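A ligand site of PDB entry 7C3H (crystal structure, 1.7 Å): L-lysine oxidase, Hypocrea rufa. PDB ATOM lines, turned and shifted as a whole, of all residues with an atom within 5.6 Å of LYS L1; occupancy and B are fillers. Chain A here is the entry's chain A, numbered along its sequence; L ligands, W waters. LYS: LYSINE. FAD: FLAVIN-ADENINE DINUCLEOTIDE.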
ATOM      1  N   MET A  67      22.624  27.124  -2.356  1.00  0.00           N
ATOM      2  CA  MET A  67      23.675  26.318  -1.730  1.00  0.00           C
ATOM      3  C   MET A  67      24.293  25.254  -2.628  1.00  0.00           C
ATOM      4  O   MET A  67      25.388  24.802  -2.286  1.00  0.00           O
ATOM      5  CB  MET A  67      23.145  25.627  -0.457  1.00  0.00           C
ATOM      6  CG  MET A  67      22.272  24.412  -0.718  1.00  0.00           C
ATOM      7  SD  MET A  67      21.489  23.860   0.820  1.00  0.00           S
ATOM      8  CE  MET A  67      20.452  22.443   0.307  1.00  0.00           C
ATOM      9  N   ARG A  68      23.687  24.838  -3.755  1.00  0.00           N
ATOM     10  CA  ARG A  68      24.203  23.694  -4.510  1.00  0.00           C
ATOM     11  C   ARG A  68      23.996  23.932  -6.001  1.00  0.00           C
ATOM     12  O   ARG A  68      22.987  24.517  -6.394  1.00  0.00           O
ATOM     13  CB  ARG A  68      23.478  22.380  -4.153  1.00  0.00           C
ATOM     14  CG  ARG A  68      21.902  22.470  -4.283  1.00  0.00           C
ATOM     15  CD  ARG A  68      21.232  21.192  -3.732  1.00  0.00           C
ATOM     16  NE  ARG A  68      19.779  21.341  -3.667  1.00  0.00           N
ATOM     17  CZ  ARG A  68      18.988  20.488  -3.009  1.00  0.00           C
ATOM     18  NH1 ARG A  68      19.518  19.400  -2.435  1.00  0.00           N
ATOM     19  NH2 ARG A  68      17.703  20.682  -2.971  1.00  0.00           N
ATOM     20  N   ASP A 212      12.082  20.831 -12.708  1.00  0.00           N
ATOM     21  CA  ASP A 212      12.735  20.417 -11.471  1.00  0.00           C
ATOM     22  C   ASP A 212      13.414  19.059 -11.634  1.00  0.00           C
ATOM     23  O   ASP A 212      14.548  18.847 -11.115  1.00  0.00           O
ATOM     24  CB  ASP A 212      11.710  20.358 -10.349  1.00  0.00           C
ATOM     25  CG  ASP A 212      11.408  21.726  -9.770  1.00  0.00           C
ATOM     26  OD1 ASP A 212      12.049  22.721 -10.141  1.00  0.00           O
ATOM     27  OD2 ASP A 212      10.564  21.774  -8.836  1.00  0.00           O
ATOM     28  N   PHE A 216      17.297  18.097 -11.019  1.00  0.00           N
ATOM     29  CA  PHE A 216      17.708  17.222  -9.946  1.00  0.00           C
ATOM     30  C   PHE A 216      18.098  15.840 -10.420  1.00  0.00           C
ATOM     31  O   PHE A 216      18.884  15.178  -9.744  1.00  0.00           O
ATOM     32  CB  PHE A 216      16.562  17.089  -8.933  1.00  0.00           C
ATOM     33  CG  PHE A 216      16.447  18.288  -8.023  1.00  0.00           C
ATOM     34  CD1 PHE A 216      17.498  18.647  -7.198  1.00  0.00           C
ATOM     35  CD2 PHE A 216      15.262  19.022  -7.989  1.00  0.00           C
ATOM     36  CE1 PHE A 216      17.416  19.729  -6.362  1.00  0.00           C
ATOM     37  CE2 PHE A 216      15.131  20.136  -7.081  1.00  0.00           C
ATOM     38  CZ  PHE A 216      16.239  20.490  -6.285  1.00  0.00           C
ATOM     39  N   TRP A 224      27.850  17.719  -8.806  1.00  0.00           N
ATOM     40  CA  TRP A 224      27.322  18.873  -8.102  1.00  0.00           C
ATOM     41  C   TRP A 224      28.421  19.576  -7.326  1.00  0.00           C
ATOM     42  O   TRP A 224      29.365  18.943  -6.843  1.00  0.00           O
ATOM     43  CB  TRP A 224      26.197  18.462  -7.145  1.00  0.00           C
ATOM     44  CG  TRP A 224      24.915  18.013  -7.816  1.00  0.00           C
ATOM     45  CD1 TRP A 224      24.691  16.805  -8.438  1.00  0.00           C
ATOM     46  CD2 TRP A 224      23.660  18.703  -7.821  1.00  0.00           C
ATOM     47  NE1 TRP A 224      23.378  16.751  -8.940  1.00  0.00           N
ATOM     48  CE2 TRP A 224      22.728  17.902  -8.546  1.00  0.00           C
ATOM     49  CE3 TRP A 224      23.238  19.960  -7.316  1.00  0.00           C
ATOM     50  CZ2 TRP A 224      21.391  18.283  -8.728  1.00  0.00           C
ATOM     51  CZ3 TRP A 224      21.917  20.351  -7.539  1.00  0.00           C
ATOM     52  CH2 TRP A 224      21.023  19.519  -8.251  1.00  0.00           C
ATOM     53  N   ASP A 315       6.643  29.735  -4.548  1.00  0.00           N
ATOM     54  CA  ASP A 315       6.696  28.723  -3.511  1.00  0.00           C
ATOM     55  C   ASP A 315       7.264  29.370  -2.237  1.00  0.00           C
ATOM     56  O   ASP A 315       7.808  30.480  -2.293  1.00  0.00           O
ATOM     57  CB  ASP A 315       7.630  27.578  -3.916  1.00  0.00           C
ATOM     58  CG  ASP A 315       7.370  26.291  -3.123  1.00  0.00           C
ATOM     59  OD1 ASP A 315       6.364  26.229  -2.383  1.00  0.00           O
ATOM     60  OD2 ASP A 315       8.185  25.384  -3.279  1.00  0.00           O
ATOM     61  N   TYR A 369      14.895  21.166   5.589  1.00  0.00           N
ATOM     62  CA  TYR A 369      14.798  22.025   4.438  1.00  0.00           C
ATOM     63  C   TYR A 369      13.472  21.665   3.811  1.00  0.00           C
ATOM     64  O   TYR A 369      13.293  20.527   3.303  1.00  0.00           O
ATOM     65  CB  TYR A 369      15.955  21.784   3.461  1.00  0.00           C
ATOM     66  CG  TYR A 369      15.871  22.539   2.161  1.00  0.00           C
ATOM     67  CD1 TYR A 369      15.225  23.810   2.050  1.00  0.00           C
ATOM     68  CD2 TYR A 369      16.404  21.991   1.047  1.00  0.00           C
ATOM     69  CE1 TYR A 369      15.156  24.515   0.787  1.00  0.00           C
ATOM     70  CE2 TYR A 369      16.278  22.641  -0.216  1.00  0.00           C
ATOM     71  CZ  TYR A 369      15.700  23.894  -0.326  1.00  0.00           C
ATOM     72  OH  TYR A 369      15.601  24.532  -1.557  1.00  0.00           O
ATOM     73  N   TRP A 371       9.700  22.953   1.521  1.00  0.00           N
ATOM     74  CA  TRP A 371       9.041  23.778   0.507  1.00  0.00           C
ATOM     75  C   TRP A 371       7.546  23.804   0.801  1.00  0.00           C
ATOM     76  O   TRP A 371       7.036  23.000   1.591  1.00  0.00           O
ATOM     77  CB  TRP A 371       9.227  23.205  -0.926  1.00  0.00           C
ATOM     78  CG  TRP A 371      10.594  23.157  -1.424  1.00  0.00           C
ATOM     79  CD1 TRP A 371      11.610  24.026  -1.123  1.00  0.00           C
ATOM     80  CD2 TRP A 371      11.166  22.184  -2.342  1.00  0.00           C
ATOM     81  NE1 TRP A 371      12.778  23.643  -1.771  1.00  0.00           N
ATOM     82  CE2 TRP A 371      12.531  22.507  -2.517  1.00  0.00           C
ATOM     83  CE3 TRP A 371      10.640  21.045  -2.991  1.00  0.00           C
ATOM     84  CZ2 TRP A 371      13.385  21.785  -3.366  1.00  0.00           C
ATOM     85  CZ3 TRP A 371      11.485  20.325  -3.863  1.00  0.00           C
ATOM     86  CH2 TRP A 371      12.858  20.699  -4.022  1.00  0.00           C
ATOM     87  N   PHE A 439      10.781  31.628  -4.134  1.00  0.00           N
ATOM     88  CA  PHE A 439      11.160  31.729  -5.537  1.00  0.00           C
ATOM     89  C   PHE A 439       9.906  31.402  -6.339  1.00  0.00           C
ATOM     90  O   PHE A 439       8.963  30.759  -5.837  1.00  0.00           O
ATOM     91  CB  PHE A 439      12.303  30.756  -5.942  1.00  0.00           C
ATOM     92  CG  PHE A 439      12.316  29.431  -5.204  1.00  0.00           C
ATOM     93  CD1 PHE A 439      11.286  28.530  -5.321  1.00  0.00           C
ATOM     94  CD2 PHE A 439      13.429  29.085  -4.382  1.00  0.00           C
ATOM     95  CE1 PHE A 439      11.289  27.315  -4.634  1.00  0.00           C
ATOM     96  CE2 PHE A 439      13.423  27.872  -3.717  1.00  0.00           C
ATOM     97  CZ  PHE A 439      12.303  27.011  -3.826  1.00  0.00           C
ATOM     98  N   ALA A 440       9.932  31.795  -7.598  1.00  0.00           N
ATOM     99  CA  ALA A 440       8.841  31.458  -8.506  1.00  0.00           C
ATOM    100  C   ALA A 440       8.680  29.977  -8.678  1.00  0.00           C
ATOM    101  O   ALA A 440       9.657  29.232  -8.775  1.00  0.00           O
ATOM    102  CB  ALA A 440       9.141  32.113  -9.867  1.00  0.00           C
ATOM    103  N   LEU A 441       7.419  29.539  -8.668  1.00  0.00           N
ATOM    104  CA  LEU A 441       7.118  28.166  -9.015  1.00  0.00           C
ATOM    105  C   LEU A 441       5.703  28.256  -9.581  1.00  0.00           C
ATOM    106  O   LEU A 441       4.725  28.318  -8.844  1.00  0.00           O
ATOM    107  CB  LEU A 441       7.214  27.229  -7.815  1.00  0.00           C
ATOM    108  CG  LEU A 441       7.221  25.727  -8.114  1.00  0.00           C
ATOM    109  CD1 LEU A 441       7.642  24.914  -6.839  1.00  0.00           C
ATOM    110  CD2 LEU A 441       5.942  25.164  -8.728  1.00  0.00           C
ATOM    111  N   HIS A 474      13.526  29.107 -12.955  1.00  0.00           N
ATOM    112  CA  HIS A 474      13.159  29.523 -11.611  1.00  0.00           C
ATOM    113  C   HIS A 474      13.989  28.839 -10.544  1.00  0.00           C
ATOM    114  O   HIS A 474      14.334  27.672 -10.638  1.00  0.00           O
ATOM    115  CB  HIS A 474      11.699  29.164 -11.443  1.00  0.00           C
ATOM    116  CG  HIS A 474      10.827  29.979 -12.351  1.00  0.00           C
ATOM    117  ND1 HIS A 474       9.550  29.607 -12.685  1.00  0.00           N
ATOM    118  CD2 HIS A 474      11.061  31.170 -12.941  1.00  0.00           C
ATOM    119  CE1 HIS A 474       9.014  30.550 -13.476  1.00  0.00           C
ATOM    120  NE2 HIS A 474       9.907  31.521 -13.641  1.00  0.00           N
ATOM    121  N   ALA A 475      14.202  29.571  -9.448  1.00  0.00           N
ATOM    122  CA  ALA A 475      14.792  29.011  -8.227  1.00  0.00           C
ATOM    123  C   ALA A 475      16.227  28.540  -8.403  1.00  0.00           C
ATOM    124  O   ALA A 475      16.718  27.752  -7.583  1.00  0.00           O
ATOM    125  CB  ALA A 475      13.941  27.854  -7.657  1.00  0.00           C
ATOM    126  N   TRP A 476      16.955  29.056  -9.386  1.00  0.00           N
ATOM    127  CA  TRP A 476      18.391  28.858  -9.489  1.00  0.00           C
ATOM    128  C   TRP A 476      19.078  30.179  -9.831  1.00  0.00           C
ATOM    129  O   TRP A 476      18.487  31.075 -10.471  1.00  0.00           O
ATOM    130  CB  TRP A 476      18.735  27.799 -10.582  1.00  0.00           C
ATOM    131  CG  TRP A 476      18.093  26.483 -10.319  1.00  0.00           C
ATOM    132  CD1 TRP A 476      16.896  26.042 -10.807  1.00  0.00           C
ATOM    133  CD2 TRP A 476      18.648  25.415  -9.563  1.00  0.00           C
ATOM    134  NE1 TRP A 476      16.633  24.755 -10.336  1.00  0.00           N
ATOM    135  CE2 TRP A 476      17.702  24.359  -9.563  1.00  0.00           C
ATOM    136  CE3 TRP A 476      19.870  25.239  -8.868  1.00  0.00           C
ATOM    137  CZ2 TRP A 476      17.932  23.120  -8.916  1.00  0.00           C
ATOM    138  CZ3 TRP A 476      20.085  24.044  -8.201  1.00  0.00           C
ATOM    139  CH2 TRP A 476      19.116  22.976  -8.233  1.00  0.00           C
HETATM  140  N   LYS L   1      17.347  25.438  -6.366  1.00  0.00           N
HETATM  141  CA  LYS L   1      16.547  25.018  -5.186  1.00  0.00           C
HETATM  142  C   LYS L   1      17.180  23.752  -4.605  1.00  0.00           C
HETATM  143  O   LYS L   1      18.229  23.263  -5.084  1.00  0.00           O
HETATM  144  CB  LYS L   1      15.069  24.797  -5.547  1.00  0.00           C
HETATM  145  CG  LYS L   1      14.801  23.711  -6.624  1.00  0.00           C
HETATM  146  CD  LYS L   1      13.258  23.342  -6.781  1.00  0.00           C
HETATM  147  CE  LYS L   1      12.460  24.579  -7.334  1.00  0.00           C
HETATM  148  NZ  LYS L   1      10.966  24.260  -7.470  1.00  0.00           N
HETATM  149  OXT LYS L   1      16.659  23.227  -3.623  1.00  0.00           O
HETATM  150  PA  FAD L   2      16.914  38.522  -5.027  1.00  0.00           P
HETATM  151  O1A FAD L   2      15.622  38.469  -4.363  1.00  0.00           O
HETATM  152  O2A FAD L   2      17.997  37.691  -4.518  1.00  0.00           O
HETATM  153  O5B FAD L   2      17.469  39.972  -5.108  1.00  0.00           O
HETATM  154  C5B FAD L   2      16.588  41.105  -5.202  1.00  0.00           C
HETATM  155  C4B FAD L   2      17.031  42.178  -4.223  1.00  0.00           C
HETATM  156  O4B FAD L   2      16.062  43.257  -4.301  1.00  0.00           O
HETATM  157  C3B FAD L   2      17.105  41.755  -2.751  1.00  0.00           C
HETATM  158  O3B FAD L   2      18.412  42.015  -2.221  1.00  0.00           O
HETATM  159  C2B FAD L   2      15.976  42.565  -2.096  1.00  0.00           C
HETATM  160  O2B FAD L   2      16.299  42.838  -0.730  1.00  0.00           O
HETATM  161  C1B FAD L   2      15.951  43.802  -2.993  1.00  0.00           C
HETATM  162  N9A FAD L   2      14.709  44.569  -2.925  1.00  0.00           N
HETATM  163  C8A FAD L   2      13.439  44.096  -2.680  1.00  0.00           C
HETATM  164  N7A FAD L   2      12.523  45.039  -2.688  1.00  0.00           N
HETATM  165  C5A FAD L   2      13.223  46.197  -2.985  1.00  0.00           C
HETATM  166  C6A FAD L   2      12.844  47.542  -3.103  1.00  0.00           C
HETATM  167  N6A FAD L   2      11.572  47.949  -3.011  1.00  0.00           N
HETATM  168  N1A FAD L   2      13.810  48.461  -3.351  1.00  0.00           N
HETATM  169  C2A FAD L   2      15.076  48.048  -3.435  1.00  0.00           C
HETATM  170  N3A FAD L   2      15.553  46.809  -3.333  1.00  0.00           N
HETATM  171  C4A FAD L   2      14.582  45.939  -3.100  1.00  0.00           C
HETATM  172  N1  FAD L   2      19.976  28.702  -6.666  1.00  0.00           N
HETATM  173  C2  FAD L   2      20.957  27.841  -7.043  1.00  0.00           C
HETATM  174  O2  FAD L   2      21.580  27.963  -8.148  1.00  0.00           O
HETATM  175  N3  FAD L   2      21.263  26.769  -6.192  1.00  0.00           N
HETATM  176  C4  FAD L   2      20.608  26.487  -5.020  1.00  0.00           C
HETATM  177  O4  FAD L   2      20.956  25.581  -4.270  1.00  0.00           O
HETATM  178  C4X FAD L   2      19.537  27.354  -4.678  1.00  0.00           C
HETATM  179  N5  FAD L   2      18.826  27.066  -3.563  1.00  0.00           N
HETATM  180  C5X FAD L   2      17.951  28.010  -3.101  1.00  0.00           C
HETATM  181  C6  FAD L   2      17.301  27.795  -1.871  1.00  0.00           C
HETATM  182  C7  FAD L   2      16.353  28.712  -1.405  1.00  0.00           C
HETATM  183  C7M FAD L   2      15.624  28.445  -0.100  1.00  0.00           C
HETATM  184  C8  FAD L   2      16.067  29.842  -2.174  1.00  0.00           C
HETATM  185  C8M FAD L   2      15.041  30.838  -1.703  1.00  0.00           C
HETATM  186  C9  FAD L   2      16.719  30.062  -3.382  1.00  0.00           C
HETATM  187  C9A FAD L   2      17.660  29.164  -3.856  1.00  0.00           C
HETATM  188  N10 FAD L   2      18.293  29.331  -5.125  1.00  0.00           N
HETATM  189  C10 FAD L   2      19.287  28.450  -5.535  1.00  0.00           C
HETATM  190  C1' FAD L   2      17.905  30.430  -6.015  1.00  0.00           C
HETATM  191  C2' FAD L   2      18.770  31.669  -5.933  1.00  0.00           C
HETATM  192  O2' FAD L   2      19.078  31.862  -4.534  1.00  0.00           O
HETATM  193  C3' FAD L   2      17.954  32.834  -6.482  1.00  0.00           C
HETATM  194  O3' FAD L   2      17.360  32.467  -7.750  1.00  0.00           O
HETATM  195  C4' FAD L   2      18.735  34.121  -6.697  1.00  0.00           C
HETATM  196  O4' FAD L   2      19.606  34.317  -5.584  1.00  0.00           O
HETATM  197  C5' FAD L   2      17.778  35.275  -6.816  1.00  0.00           C
HETATM  198  O5' FAD L   2      18.502  36.439  -7.246  1.00  0.00           O
HETATM  199  P   FAD L   2      17.750  37.713  -7.743  1.00  0.00           P
HETATM  200  O1P FAD L   2      16.875  37.244  -8.915  1.00  0.00           O
HETATM  201  O2P FAD L   2      18.794  38.802  -7.894  1.00  0.00           O
HETATM  202  O3P FAD L   2      16.697  38.081  -6.551  1.00  0.00           O
HETATM  203  O   HOH W   1      10.105  23.979  -4.728  1.00  0.00           O
HETATM  204  O   HOH W   2      10.564  26.494  -8.835  1.00  0.00           O
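OXT of LYS L1 is in salt-bridge range of NH2 of Arg 68 (2.8 Å). O3' of FAD L2 lies within hydrogen-bond range of O of Trp 476, 3.3 Å away. NZ of LYS L1 is in salt-bridge range of OD2 of Asp 212, 2.9 Å away. An oxygen (OXT) of LYS L1 sits at hydrogen-bond distance from the side-chain hydroxyl of Tyr 369 (2.7 Å). The backbone carbonyl oxygen of Ala 475 lies within hydrogen-bond range of a nitrogen (N) of LYS L1, at 2.7 Å. N of Arg 68 is in hydrogen-bond range of O4 of FAD L2 (2.9 Å). O4 of FAD L2 lies within hydrogen-bond range of N of Met 67, at 3.0 Å. N3 of FAD L2 is in hydrogen-bond range of O of Arg 68 (2.8 Å).
The backbone carbonyl oxygen (O) of Phe 439 sits at hydrogen-bond distance from the backbone NH (N) of Asp 315, 2.8 Å away. NE1 of Trp 371 sits at hydrogen-bond distance from OH of Tyr 369 (3.0 Å).
Merely in contact with LYS L1: Trp 476 (3.3 Å), Leu 441 (3.4 Å), Phe 216 (3.5 Å), Trp 371 (3.6 Å) and Phe 439 (3.9 Å). Hydrophobic or aromatic side chains within 4 Å of LYS L1: Phe 216, Tyr 369, Trp 371, Phe 439, Leu 441, Ala 475 and Trp 476.
Water W2 bridges a nitrogen (NZ) of LYS L1 and the backbone carbonyl oxygen (O) of Ala 440. Water W1 lies within hydrogen-bond range of the side-chain carboxylate of Asp 315 (2.8 Å) and a nitrogen (NZ) of LYS L1 (2.9 Å).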
